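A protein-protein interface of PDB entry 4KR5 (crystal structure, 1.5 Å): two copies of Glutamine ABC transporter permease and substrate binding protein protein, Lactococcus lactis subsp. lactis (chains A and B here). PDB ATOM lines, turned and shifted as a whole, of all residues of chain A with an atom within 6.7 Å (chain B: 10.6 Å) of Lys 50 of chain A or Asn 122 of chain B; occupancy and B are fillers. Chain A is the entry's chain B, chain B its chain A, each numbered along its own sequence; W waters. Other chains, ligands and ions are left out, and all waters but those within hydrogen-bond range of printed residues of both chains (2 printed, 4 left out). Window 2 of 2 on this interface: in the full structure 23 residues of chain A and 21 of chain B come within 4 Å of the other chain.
O of Trp 51 of chain A is in hydrogen-bond range of ND2 of Asn 122 of chain B, at 2.9 Å.
ND2 of Asn 122 of chain B lies within hydrogen-bond range of OD1 of Asn 52 of chain A (2.5 Å).
The backbone carbonyl oxygen (O) of Lys 121 of chain B sits at hydrogen-bond distance from the side-chain hydroxyl (OG1) of Thr 124 of chain B (2.8 Å).
OG1 of Thr 124 of chain B sits close to N of Ser 126 of chain B (3.4 Å).
The side-chain hydroxyl (OG1) of Thr 124 of chain B lies within hydrogen-bond range of the backbone NH (N) of Phe 127 of chain B, 3.1 Å away.
The backbone NH (N) of Lys 50 of chain A is in hydrogen-bond range of the backbone carbonyl oxygen (O) of Tyr 10 of chain A.
The backbone NH of Ile 12 of chain A lies within hydrogen-bond range of the backbone carbonyl oxygen of Lys 50 of chain A (2.8 Å).
N of Asn 52 of chain A lies within hydrogen-bond range of O of Ile 12 of chain A (2.8 Å).
Among the printed residues, merely in contact across the chains: Ile 54 of chain A with Asn 122 of chain B (3.3 Å), Asn 52 of chain A with Gly 123 of chain B (3.5 Å), Lys 50 of chain A with Asn 122 of chain B (3.9 Å), Ile 54 of chain A with Thr 124 of chain B (3.9 Å) and Ile 54 of chain A with Gly 123 of chain B (3.9 Å).
Of the printed residues of chain B, Lys 50 of chain A touches Asn 122 (3.9 Å).
Printed residues of chain A within 4 Å of Asn 122 of chain B: Lys 50, Trp 51, Asn 52 and Ile 54.
No residue of chain B comes within 4 Å of Thr 11 of chain A.
No residue of chain B comes within 4 Å of Ile 12 of chain A.
No residue of chain B comes within 4 Å of Leu 49 of chain A.
Of the printed residues of chain B, Trp 51 of chain A touches Asn 122 (2.9 Å).
Printed residues of chain A within 4 Å of Gly 123 of chain B: Asn 52 (3.5 Å) and Ile 54 (3.9 Å).
Of the printed residues of chain A, Thr 124 of chain B touches Ile 54 (3.9 Å).
Printed residues of chain B within 4 Å of Ile 54 of chain A: Asn 122, Gly 123 and Thr 124.
Ala 120 of chain B touches none of the printed residues of chain A.
The nearest printed residue of chain B that does not touch Lys 50 of chain A is Phe 127 of chain B (4.3 Å).
Of the 26 printed residues of chain B, 3 touch a printed residue of chain A.
Printed residues of chain B that touch a printed residue of chain A: Asn 122, Gly 123 and Thr 124.
Among the printed residues, no Asp or Glu carboxylate lies within 4 Å of a Lys or Arg side-chain nitrogen of the other chain.
No position is printed for both chains.
Of the 7 pairs that touch across the chains among the printed residues, none has its exchanged pair printed and touching as well.
Water W1 lies within hydrogen-bond range of the backbone carbonyl oxygen (O) of Trp 51 of chain A (2.7 Å) and the side-chain amide nitrogen (ND2) of Asn 122 of chain B (3.5 Å).
Water W2 bridges the backbone carbonyl oxygen of Gly 123 of chain B (2.8 Å) and the side-chain amide nitrogen of Asn 52 of chain A (2.8 Å).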
ATOM      1  N   VAL A   9      12.631 -22.916  37.347  1.00  0.00           N
ATOM      2  CA  VAL A   9      11.774 -21.779  37.690  1.00  0.00           C
ATOM      3  C   VAL A   9      10.322 -22.135  37.401  1.00  0.00           C
ATOM      4  O   VAL A   9      10.022 -22.781  36.391  1.00  0.00           O
ATOM      5  CB  VAL A   9      12.149 -20.498  36.905  1.00  0.00           C
ATOM      6  CG1 VAL A   9      11.277 -19.335  37.332  1.00  0.00           C
ATOM      7  CG2 VAL A   9      13.611 -20.130  37.126  1.00  0.00           C
ATOM      8  N   TYR A  10       9.428 -21.717  38.298  1.00  0.00           N
ATOM      9  CA  TYR A  10       7.990 -21.916  38.115  1.00  0.00           C
ATOM     10  C   TYR A  10       7.355 -20.596  37.684  1.00  0.00           C
ATOM     11  O   TYR A  10       7.646 -19.528  38.245  1.00  0.00           O
ATOM     12  CB  TYR A  10       7.332 -22.437  39.402  1.00  0.00           C
ATOM     13  CG  TYR A  10       7.685 -23.882  39.749  1.00  0.00           C
ATOM     14  CD1 TYR A  10       6.926 -24.933  39.262  1.00  0.00           C
ATOM     15  CD2 TYR A  10       8.785 -24.193  40.564  1.00  0.00           C
ATOM     16  CE1 TYR A  10       7.235 -26.252  39.577  1.00  0.00           C
ATOM     17  CE2 TYR A  10       9.101 -25.514  40.879  1.00  0.00           C
ATOM     18  CZ  TYR A  10       8.328 -26.530  40.385  1.00  0.00           C
ATOM     19  OH  TYR A  10       8.644 -27.825  40.691  1.00  0.00           O
ATOM     20  N   THR A  11       6.492 -20.680  36.672  1.00  0.00           N
ATOM     21  CA  THR A  11       5.809 -19.523  36.127  1.00  0.00           C
ATOM     22  C   THR A  11       4.462 -19.360  36.825  1.00  0.00           C
ATOM     23  O   THR A  11       3.664 -20.284  36.868  1.00  0.00           O
ATOM     24  CB  THR A  11       5.611 -19.680  34.592  1.00  0.00           C
ATOM     25  OG1 THR A  11       6.899 -19.706  33.968  1.00  0.00           O
ATOM     26  CG2 THR A  11       4.793 -18.517  34.009  1.00  0.00           C
ATOM     27  N   ILE A  12       4.241 -18.181  37.389  1.00  0.00           N
ATOM     28  CA  ILE A  12       2.999 -17.880  38.101  1.00  0.00           C
ATOM     29  C   ILE A  12       2.234 -16.790  37.364  1.00  0.00           C
ATOM     30  O   ILE A  12       2.750 -15.686  37.173  1.00  0.00           O
ATOM     31  CB  ILE A  12       3.298 -17.378  39.544  1.00  0.00           C
ATOM     32  CG1 ILE A  12       4.266 -18.333  40.273  1.00  0.00           C
ATOM     33  CG2 ILE A  12       1.980 -17.195  40.365  1.00  0.00           C
ATOM     34  CD1 ILE A  12       3.737 -19.757  40.428  1.00  0.00           C
ATOM     35  N   ALA A  13       0.993 -17.101  36.981  1.00  0.00           N
ATOM     36  CA  ALA A  13       0.121 -16.111  36.343  1.00  0.00           C
ATOM     37  C   ALA A  13      -0.737 -15.408  37.383  1.00  0.00           C
ATOM     38  O   ALA A  13      -1.148 -16.002  38.375  1.00  0.00           O
ATOM     39  CB  ALA A  13      -0.746 -16.752  35.285  1.00  0.00           C
ATOM     40  N   LYS A  48      12.141 -21.175  42.858  1.00  0.00           N
ATOM     41  CA  LYS A  48      12.269 -19.904  42.127  1.00  0.00           C
ATOM     42  C   LYS A  48      11.009 -19.664  41.298  1.00  0.00           C
ATOM     43  O   LYS A  48      10.417 -20.621  40.800  1.00  0.00           O
ATOM     44  CB  LYS A  48      13.474 -19.914  41.191  1.00  0.00           C
ATOM     45  CG  LYS A  48      14.834 -20.125  41.891  1.00  0.00           C
ATOM     46  CD  LYS A  48      15.197 -18.956  42.793  1.00  0.00           C
ATOM     47  CE  LYS A  48      16.636 -19.044  43.310  1.00  0.00           C
ATOM     48  NZ  LYS A  48      16.836 -20.077  44.374  1.00  0.00           N
ATOM     49  N   LEU A  49      10.635 -18.393  41.159  1.00  0.00           N
ATOM     50  CA  LEU A  49       9.411 -17.989  40.448  1.00  0.00           C
ATOM     51  C   LEU A  49       9.667 -16.964  39.369  1.00  0.00           C
ATOM     52  O   LEU A  49      10.600 -16.165  39.440  1.00  0.00           O
ATOM     53  CB  LEU A  49       8.422 -17.340  41.421  1.00  0.00           C
ATOM     54  CG  LEU A  49       8.010 -18.081  42.683  1.00  0.00           C
ATOM     55  CD1 LEU A  49       7.100 -17.178  43.477  1.00  0.00           C
ATOM     56  CD2 LEU A  49       7.361 -19.409  42.366  1.00  0.00           C
ATOM     57  N   LYS A  50       8.761 -16.968  38.393  1.00  0.00           N
ATOM     58  CA  LYS A  50       8.669 -15.920  37.388  1.00  0.00           C
ATOM     59  C   LYS A  50       7.193 -15.526  37.319  1.00  0.00           C
ATOM     60  O   LYS A  50       6.330 -16.385  37.198  1.00  0.00           O
ATOM     61  CB  LYS A  50       9.158 -16.450  36.040  1.00  0.00           C
ATOM     62  CG  LYS A  50       9.155 -15.452  34.901  1.00  0.00           C
ATOM     63  CD  LYS A  50       9.599 -16.144  33.624  1.00  0.00           C
ATOM     64  CE  LYS A  50       9.531 -15.242  32.420  1.00  0.00           C
ATOM     65  NZ  LYS A  50       9.482 -16.060  31.173  1.00  0.00           N
ATOM     66  N   TRP A  51       6.906 -14.232  37.430  1.00  0.00           N
ATOM     67  CA  TRP A  51       5.505 -13.753  37.477  1.00  0.00           C
ATOM     68  C   TRP A  51       5.045 -13.235  36.131  1.00  0.00           C
ATOM     69  O   TRP A  51       5.783 -12.509  35.461  1.00  0.00           O
ATOM     70  CB  TRP A  51       5.373 -12.601  38.469  1.00  0.00           C
ATOM     71  CG  TRP A  51       5.467 -12.991  39.909  1.00  0.00           C
ATOM     72  CD1 TRP A  51       6.604 -13.136  40.651  1.00  0.00           C
ATOM     73  CD2 TRP A  51       4.380 -13.279  40.773  1.00  0.00           C
ATOM     74  NE1 TRP A  51       6.285 -13.504  41.935  1.00  0.00           N
ATOM     75  CE2 TRP A  51       4.922 -13.577  42.044  1.00  0.00           C
ATOM     76  CE3 TRP A  51       2.996 -13.299  40.611  1.00  0.00           C
ATOM     77  CZ2 TRP A  51       4.123 -13.927  43.131  1.00  0.00           C
ATOM     78  CZ3 TRP A  51       2.205 -13.612  41.696  1.00  0.00           C
ATOM     79  CH2 TRP A  51       2.775 -13.937  42.945  1.00  0.00           C
ATOM     80  N   ASN A  52       3.804 -13.564  35.765  1.00  0.00           N
ATOM     81  CA  ASN A  52       3.176 -13.043  34.555  1.00  0.00           C
ATOM     82  C   ASN A  52       1.885 -12.321  34.981  1.00  0.00           C
ATOM     83  O   ASN A  52       0.892 -12.981  35.258  1.00  0.00           O
ATOM     84  CB  ASN A  52       2.784 -14.195  33.619  1.00  0.00           C
ATOM     85  CG  ASN A  52       3.971 -14.939  33.031  1.00  0.00           C
ATOM     86  OD1 ASN A  52       5.120 -14.478  33.066  1.00  0.00           O
ATOM     87  ND2 ASN A  52       3.681 -16.091  32.431  1.00  0.00           N
ATOM     88  N   PHE A  53       1.903 -10.986  35.038  1.00  0.00           N
ATOM     89  CA  PHE A  53       0.753 -10.238  35.524  1.00  0.00           C
ATOM     90  C   PHE A  53      -0.141  -9.889  34.351  1.00  0.00           C
ATOM     91  O   PHE A  53      -0.012  -8.808  33.775  1.00  0.00           O
ATOM     92  CB  PHE A  53       1.193  -8.974  36.268  1.00  0.00           C
ATOM     93  CG  PHE A  53       1.972  -9.262  37.529  1.00  0.00           C
ATOM     94  CD1 PHE A  53       1.309  -9.624  38.703  1.00  0.00           C
ATOM     95  CD2 PHE A  53       3.362  -9.196  37.539  1.00  0.00           C
ATOM     96  CE1 PHE A  53       2.026  -9.919  39.871  1.00  0.00           C
ATOM     97  CE2 PHE A  53       4.082  -9.474  38.699  1.00  0.00           C
ATOM     98  CZ  PHE A  53       3.415  -9.854  39.865  1.00  0.00           C
ATOM     99  N   ILE A  54      -1.025 -10.811  33.980  1.00  0.00           N
ATOM    100  CA  ILE A  54      -1.717 -10.730  32.689  1.00  0.00           C
ATOM    101  C   ILE A  54      -3.229 -10.491  32.761  1.00  0.00           C
ATOM    102  O   ILE A  54      -3.847 -10.164  31.739  1.00  0.00           O
ATOM    103  CB  ILE A  54      -1.417 -11.971  31.841  1.00  0.00           C
ATOM    104  CG1 ILE A  54      -1.750 -13.245  32.616  1.00  0.00           C
ATOM    105  CG2 ILE A  54       0.054 -11.971  31.439  1.00  0.00           C
ATOM    106  CD1 ILE A  54      -1.591 -14.537  31.810  1.00  0.00           C
ATOM    107  N   LEU B 118      10.689  -6.199  18.662  1.00  0.00           N
ATOM    108  CA  LEU B 118       9.251  -6.116  18.916  1.00  0.00           C
ATOM    109  C   LEU B 118       8.954  -6.290  20.378  1.00  0.00           C
ATOM    110  O   LEU B 118       9.512  -7.170  21.038  1.00  0.00           O
ATOM    111  CB  LEU B 118       8.484  -7.186  18.155  1.00  0.00           C
ATOM    112  CG  LEU B 118       8.489  -7.059  16.634  1.00  0.00           C
ATOM    113  CD1 LEU B 118       9.646  -7.825  16.045  1.00  0.00           C
ATOM    114  CD2 LEU B 118       7.149  -7.519  16.070  1.00  0.00           C
ATOM    115  N   GLY B 119       8.020  -5.490  20.864  1.00  0.00           N
ATOM    116  CA  GLY B 119       7.546  -5.629  22.228  1.00  0.00           C
ATOM    117  C   GLY B 119       6.357  -6.564  22.368  1.00  0.00           C
ATOM    118  O   GLY B 119       5.518  -6.682  21.460  1.00  0.00           O
ATOM    119  N   ALA B 120       6.290  -7.222  23.526  1.00  0.00           N
ATOM    120  CA  ALA B 120       5.089  -7.923  23.961  1.00  0.00           C
ATOM    121  C   ALA B 120       5.026  -7.888  25.473  1.00  0.00           C
ATOM    122  O   ALA B 120       6.061  -7.786  26.134  1.00  0.00           O
ATOM    123  CB  ALA B 120       5.100  -9.367  23.476  1.00  0.00           C
ATOM    124  N   LYS B 121       3.816  -7.984  26.019  1.00  0.00           N
ATOM    125  CA  LYS B 121       3.650  -8.065  27.464  1.00  0.00           C
ATOM    126  C   LYS B 121       3.959  -9.485  27.920  1.00  0.00           C
ATOM    127  O   LYS B 121       3.496 -10.446  27.320  1.00  0.00           O
ATOM    128  CB  LYS B 121       2.237  -7.619  27.864  1.00  0.00           C
ATOM    129  CG  LYS B 121       1.981  -6.153  27.534  1.00  0.00           C
ATOM    130  CD  LYS B 121       0.616  -5.683  28.021  1.00  0.00           C
ATOM    131  CE  LYS B 121      -0.525  -6.465  27.395  1.00  0.00           C
ATOM    132  NZ  LYS B 121      -1.852  -5.914  27.798  1.00  0.00           N
ATOM    133  N   ASN B 122       4.800  -9.593  28.944  1.00  0.00           N
ATOM    134  CA  ASN B 122       5.230 -10.875  29.467  1.00  0.00           C
ATOM    135  C   ASN B 122       4.097 -11.877  29.725  1.00  0.00           C
ATOM    136  O   ASN B 122       3.120 -11.561  30.394  1.00  0.00           O
ATOM    137  CB  ASN B 122       5.990 -10.669  30.772  1.00  0.00           C
ATOM    138  CG  ASN B 122       6.494 -11.956  31.326  1.00  0.00           C
ATOM    139  OD1 ASN B 122       7.212 -12.698  30.638  1.00  0.00           O
ATOM    140  ND2 ASN B 122       6.109 -12.260  32.581  1.00  0.00           N
ATOM    141  N   GLY B 123       4.259 -13.090  29.205  1.00  0.00           N
ATOM    142  CA  GLY B 123       3.388 -14.201  29.549  1.00  0.00           C
ATOM    143  C   GLY B 123       2.070 -14.209  28.805  1.00  0.00           C
ATOM    144  O   GLY B 123       1.207 -15.027  29.108  1.00  0.00           O
ATOM    145  N   THR B 124       1.911 -13.303  27.839  1.00  0.00           N
ATOM    146  CA  THR B 124       0.707 -13.264  27.012  1.00  0.00           C
ATOM    147  C   THR B 124       0.803 -14.153  25.775  1.00  0.00           C
ATOM    148  O   THR B 124       1.884 -14.605  25.401  1.00  0.00           O
ATOM    149  CB  THR B 124       0.408 -11.861  26.517  1.00  0.00           C
ATOM    150  OG1 THR B 124       1.492 -11.399  25.686  1.00  0.00           O
ATOM    151  CG2 THR B 124       0.221 -10.895  27.697  1.00  0.00           C
ATOM    152  N   ALA B 125      -0.347 -14.399  25.148  1.00  0.00           N
ATOM    153  CA  ALA B 125      -0.382 -15.143  23.900  1.00  0.00           C
ATOM    154  C   ALA B 125       0.525 -14.489  22.854  1.00  0.00           C
ATOM    155  O   ALA B 125       1.157 -15.183  22.062  1.00  0.00           O
ATOM    156  CB  ALA B 125      -1.810 -15.237  23.384  1.00  0.00           C
ATOM    157  N   SER B 126       0.594 -13.157  22.868  1.00  0.00           N
ATOM    158  CA  SER B 126       1.409 -12.416  21.909  1.00  0.00           C
ATOM    159  C   SER B 126       2.877 -12.683  22.171  1.00  0.00           C
ATOM    160  O   SER B 126       3.664 -12.928  21.252  1.00  0.00           O
ATOM    161  CB  SER B 126       1.118 -10.908  21.980  1.00  0.00           C
ATOM    162  OG  SER B 126      -0.159 -10.590  21.446  1.00  0.00           O
ATOM    163  N   PHE B 127       3.248 -12.630  23.445  1.00  0.00           N
ATOM    164  CA  PHE B 127       4.614 -12.944  23.873  1.00  0.00           C
ATOM    165  C   PHE B 127       4.971 -14.353  23.396  1.00  0.00           C
ATOM    166  O   PHE B 127       6.010 -14.555  22.776  1.00  0.00           O
ATOM    167  CB  PHE B 127       4.661 -12.803  25.408  1.00  0.00           C
ATOM    168  CG  PHE B 127       5.884 -13.377  26.078  1.00  0.00           C
ATOM    169  CD1 PHE B 127       7.026 -12.614  26.257  1.00  0.00           C
ATOM    170  CD2 PHE B 127       5.850 -14.651  26.619  1.00  0.00           C
ATOM    171  CE1 PHE B 127       8.134 -13.143  26.927  1.00  0.00           C
ATOM    172  CE2 PHE B 127       6.951 -15.180  27.287  1.00  0.00           C
ATOM    173  CZ  PHE B 127       8.088 -14.424  27.442  1.00  0.00           C
ATOM    174  N   ASP B 128       4.110 -15.336  23.669  1.00  0.00           N
ATOM    175  CA  ASP B 128       4.405 -16.701  23.230  1.00  0.00           C
ATOM    176  C   ASP B 128       4.535 -16.775  21.709  1.00  0.00           C
ATOM    177  O   ASP B 128       5.423 -17.464  21.188  1.00  0.00           O
ATOM    178  CB  ASP B 128       3.341 -17.697  23.707  1.00  0.00           C
ATOM    179  CG  ASP B 128       3.271 -17.806  25.224  1.00  0.00           C
ATOM    180  OD1 ASP B 128       4.299 -17.568  25.896  1.00  0.00           O
ATOM    181  OD2 ASP B 128       2.178 -18.134  25.746  1.00  0.00           O
ATOM    182  N   TYR B 129       3.662 -16.067  20.991  1.00  0.00           N
ATOM    183  CA  TYR B 129       3.658 -16.158  19.546  1.00  0.00           C
ATOM    184  C   TYR B 129       4.937 -15.535  18.993  1.00  0.00           C
ATOM    185  O   TYR B 129       5.622 -16.143  18.159  1.00  0.00           O
ATOM    186  CB  TYR B 129       2.421 -15.479  18.916  1.00  0.00           C
ATOM    187  CG  TYR B 129       2.372 -15.748  17.424  1.00  0.00           C
ATOM    188  CD1 TYR B 129       3.090 -14.957  16.540  1.00  0.00           C
ATOM    189  CD2 TYR B 129       1.648 -16.827  16.905  1.00  0.00           C
ATOM    190  CE1 TYR B 129       3.085 -15.209  15.197  1.00  0.00           C
ATOM    191  CE2 TYR B 129       1.641 -17.086  15.535  1.00  0.00           C
ATOM    192  CZ  TYR B 129       2.365 -16.268  14.693  1.00  0.00           C
ATOM    193  OH  TYR B 129       2.391 -16.508  13.343  1.00  0.00           O
ATOM    194  N   LEU B 130       5.283 -14.338  19.460  1.00  0.00           N
ATOM    195  CA  LEU B 130       6.514 -13.716  18.983  1.00  0.00           C
ATOM    196  C   LEU B 130       7.728 -14.574  19.302  1.00  0.00           C
ATOM    197  O   LEU B 130       8.608 -14.718  18.475  1.00  0.00           O
ATOM    198  CB  LEU B 130       6.709 -12.305  19.546  1.00  0.00           C
ATOM    199  CG  LEU B 130       5.803 -11.201  18.970  1.00  0.00           C
ATOM    200  CD1 LEU B 130       6.113  -9.905  19.676  1.00  0.00           C
ATOM    201  CD2 LEU B 130       5.929 -11.012  17.447  1.00  0.00           C
ATOM    202  N   ASN B 131       7.785 -15.162  20.496  1.00  0.00           N
ATOM    203  CA  ASN B 131       8.955 -15.968  20.834  1.00  0.00           C
ATOM    204  C   ASN B 131       9.075 -17.168  19.892  1.00  0.00           C
ATOM    205  O   ASN B 131      10.184 -17.536  19.456  1.00  0.00           O
ATOM    206  CB  ASN B 131       8.888 -16.418  22.291  1.00  0.00           C
ATOM    207  CG  ASN B 131       9.232 -15.305  23.267  1.00  0.00           C
ATOM    208  OD1 ASN B 131       9.987 -14.379  22.954  1.00  0.00           O
ATOM    209  ND2 ASN B 131       8.673 -15.387  24.464  1.00  0.00           N
ATOM    210  N   VAL B 141      12.711 -10.160  20.752  1.00  0.00           N
ATOM    211  CA  VAL B 141      11.535  -9.807  21.546  1.00  0.00           C
ATOM    212  C   VAL B 141      11.977  -9.046  22.786  1.00  0.00           C
ATOM    213  O   VAL B 141      12.870  -9.488  23.505  1.00  0.00           O
ATOM    214  CB  VAL B 141      10.725 -11.066  21.955  1.00  0.00           C
ATOM    215  CG1 VAL B 141       9.536 -10.689  22.837  1.00  0.00           C
ATOM    216  CG2 VAL B 141      10.248 -11.822  20.726  1.00  0.00           C
ATOM    217  N   LYS B 142      11.373  -7.883  23.005  1.00  0.00           N
ATOM    218  CA  LYS B 142      11.590  -7.128  24.228  1.00  0.00           C
ATOM    219  C   LYS B 142      10.346  -7.254  25.080  1.00  0.00           C
ATOM    220  O   LYS B 142       9.237  -7.006  24.620  1.00  0.00           O
ATOM    221  CB  LYS B 142      11.912  -5.660  23.924  1.00  0.00           C
ATOM    222  CG  LYS B 142      12.096  -4.813  25.192  1.00  0.00           C
ATOM    223  CD  LYS B 142      12.762  -3.485  24.887  1.00  0.00           C
ATOM    224  CE  LYS B 142      12.898  -2.625  26.140  1.00  0.00           C
ATOM    225  NZ  LYS B 142      13.608  -3.324  27.255  1.00  0.00           N
ATOM    226  N   THR B 143      10.540  -7.650  26.333  1.00  0.00           N
ATOM    227  CA  THR B 143       9.395  -7.906  27.206  1.00  0.00           C
ATOM    228  C   THR B 143       9.036  -6.697  28.029  1.00  0.00           C
ATOM    229  O   THR B 143       9.899  -5.961  28.518  1.00  0.00           O
ATOM    230  CB  THR B 143       9.587  -9.114  28.151  1.00  0.00           C
ATOM    231  OG1 THR B 143      10.691  -8.886  29.037  1.00  0.00           O
ATOM    232  CG2 THR B 143       9.803 -10.371  27.352  1.00  0.00           C
ATOM    233  N   PHE B 144       7.726  -6.500  28.168  1.00  0.00           N
ATOM    234  CA  PHE B 144       7.187  -5.406  28.945  1.00  0.00           C
ATOM    235  C   PHE B 144       6.267  -6.002  30.012  1.00  0.00           C
ATOM    236  O   PHE B 144       5.655  -7.072  29.792  1.00  0.00           O
ATOM    237  CB  PHE B 144       6.424  -4.438  28.039  1.00  0.00           C
ATOM    238  CG  PHE B 144       7.315  -3.631  27.137  1.00  0.00           C
ATOM    239  CD1 PHE B 144       7.759  -4.152  25.930  1.00  0.00           C
ATOM    240  CD2 PHE B 144       7.722  -2.356  27.512  1.00  0.00           C
ATOM    241  CE1 PHE B 144       8.584  -3.410  25.103  1.00  0.00           C
ATOM    242  CE2 PHE B 144       8.544  -1.612  26.699  1.00  0.00           C
ATOM    243  CZ  PHE B 144       8.977  -2.136  25.482  1.00  0.00           C
ATOM    244  N   THR B 145       6.189  -5.333  31.170  1.00  0.00           N
ATOM    245  CA  THR B 145       5.300  -5.772  32.245  1.00  0.00           C
ATOM    246  C   THR B 145       4.005  -4.979  32.274  1.00  0.00           C
ATOM    247  O   THR B 145       3.086  -5.359  32.960  1.00  0.00           O
ATOM    248  CB  THR B 145       5.935  -5.666  33.633  1.00  0.00           C
ATOM    249  OG1 THR B 145       6.238  -4.300  33.910  1.00  0.00           O
ATOM    250  CG2 THR B 145       7.180  -6.514  33.725  1.00  0.00           C
ATOM    251  N   ASP B 146       3.921  -3.871  31.550  1.00  0.00           N
ATOM    252  CA  ASP B 146       2.641  -3.178  31.411  1.00  0.00           C
ATOM    253  C   ASP B 146       2.456  -2.526  30.049  1.00  0.00           C
ATOM    254  O   ASP B 146       3.422  -2.228  29.323  1.00  0.00           O
ATOM    255  CB  ASP B 146       2.419  -2.144  32.524  1.00  0.00           C
ATOM    256  CG  ASP B 146       3.365  -0.965  32.433  1.00  0.00           C
ATOM    257  OD1 ASP B 146       3.174  -0.064  31.572  1.00  0.00           O
ATOM    258  OD2 ASP B 146       4.307  -0.935  33.242  1.00  0.00           O
ATOM    259  N   ALA B 147       1.197  -2.316  29.712  1.00  0.00           N
ATOM    260  CA  ALA B 147       0.804  -1.814  28.421  1.00  0.00           C
ATOM    261  C   ALA B 147       1.327  -0.403  28.158  1.00  0.00           C
ATOM    262  O   ALA B 147       1.842  -0.119  27.071  1.00  0.00           O
ATOM    263  CB  ALA B 147      -0.717  -1.850  28.326  1.00  0.00           C
ATOM    264  N   THR B 149       3.888   1.363  29.114  1.00  0.00           N
ATOM    265  CA  THR B 149       5.298   1.465  28.765  1.00  0.00           C
ATOM    266  C   THR B 149       5.582   0.866  27.381  1.00  0.00           C
ATOM    267  O   THR B 149       6.378   1.413  26.610  1.00  0.00           O
ATOM    268  CB  THR B 149       6.173   0.765  29.817  1.00  0.00           C
ATOM    269  OG1 THR B 149       5.909   1.329  31.105  1.00  0.00           O
ATOM    270  CG2 THR B 149       7.633   0.935  29.500  1.00  0.00           C
ATOM    271  N   MET B 150       4.929  -0.247  27.067  1.00  0.00           N
ATOM    272  CA  MET B 150       5.110  -0.889  25.770  1.00  0.00           C
ATOM    273  C   MET B 150       4.638   0.045  24.646  1.00  0.00           C
ATOM    274  O   MET B 150       5.344   0.259  23.652  1.00  0.00           O
ATOM    275  CB  MET B 150       4.356  -2.232  25.712  1.00  0.00           C
ATOM    276  CG  MET B 150       4.557  -2.979  24.399  1.00  0.00           C
ATOM    277  SD  MET B 150       3.818  -4.613  24.347  1.00  0.00           S
ATOM    278  CE  MET B 150       2.056  -4.257  24.321  1.00  0.00           C
ATOM    279  N   LEU B 162       5.057  -3.939  18.046  1.00  0.00           N
ATOM    280  CA  LEU B 162       4.609  -4.733  19.194  1.00  0.00           C
ATOM    281  C   LEU B 162       3.532  -5.677  18.701  1.00  0.00           C
ATOM    282  O   LEU B 162       2.985  -5.496  17.625  1.00  0.00           O
ATOM    283  CB  LEU B 162       4.099  -3.831  20.335  1.00  0.00           C
ATOM    284  CG  LEU B 162       2.913  -2.889  20.058  1.00  0.00           C
ATOM    285  CD1 LEU B 162       1.566  -3.617  20.161  1.00  0.00           C
ATOM    286  CD2 LEU B 162       2.906  -1.669  21.006  1.00  0.00           C
ATOM    287  N   MET B 163       3.245  -6.691  19.496  1.00  0.00           N
ATOM    288  CA  MET B 163       2.105  -7.565  19.252  1.00  0.00           C
ATOM    289  C   MET B 163       1.202  -7.514  20.476  1.00  0.00           C
ATOM    290  O   MET B 163       1.681  -7.553  21.608  1.00  0.00           O
ATOM    291  CB  MET B 163       2.548  -9.006  18.984  1.00  0.00           C
ATOM    292  CG  MET B 163       1.399  -9.889  18.485  1.00  0.00           C
ATOM    293  SD  MET B 163       1.924 -11.546  18.006  1.00  0.00           S
ATOM    294  CE  MET B 163       1.252 -11.665  16.346  1.00  0.00           C
ATOM    295  N   ASP B 164      -0.101  -7.414  20.242  1.00  0.00           N
ATOM    296  CA  ASP B 164      -1.081  -7.309  21.330  1.00  0.00           C
ATOM    297  C   ASP B 164      -2.444  -7.758  20.769  1.00  0.00           C
ATOM    298  O   ASP B 164      -2.568  -8.071  19.573  1.00  0.00           O
ATOM    299  CB  ASP B 164      -1.109  -5.859  21.848  1.00  0.00           C
ATOM    300  CG  ASP B 164      -1.837  -5.681  23.203  1.00  0.00           C
ATOM    301  OD1 ASP B 164      -2.247  -6.661  23.876  1.00  0.00           O
ATOM    302  OD2 ASP B 164      -1.954  -4.505  23.629  1.00  0.00           O
HETATM  303  O   HOH W   1       6.499  -9.915  35.106  1.00  0.00           O
HETATM  304  O   HOH W   2       1.278 -16.935  31.178  1.00  0.00           O
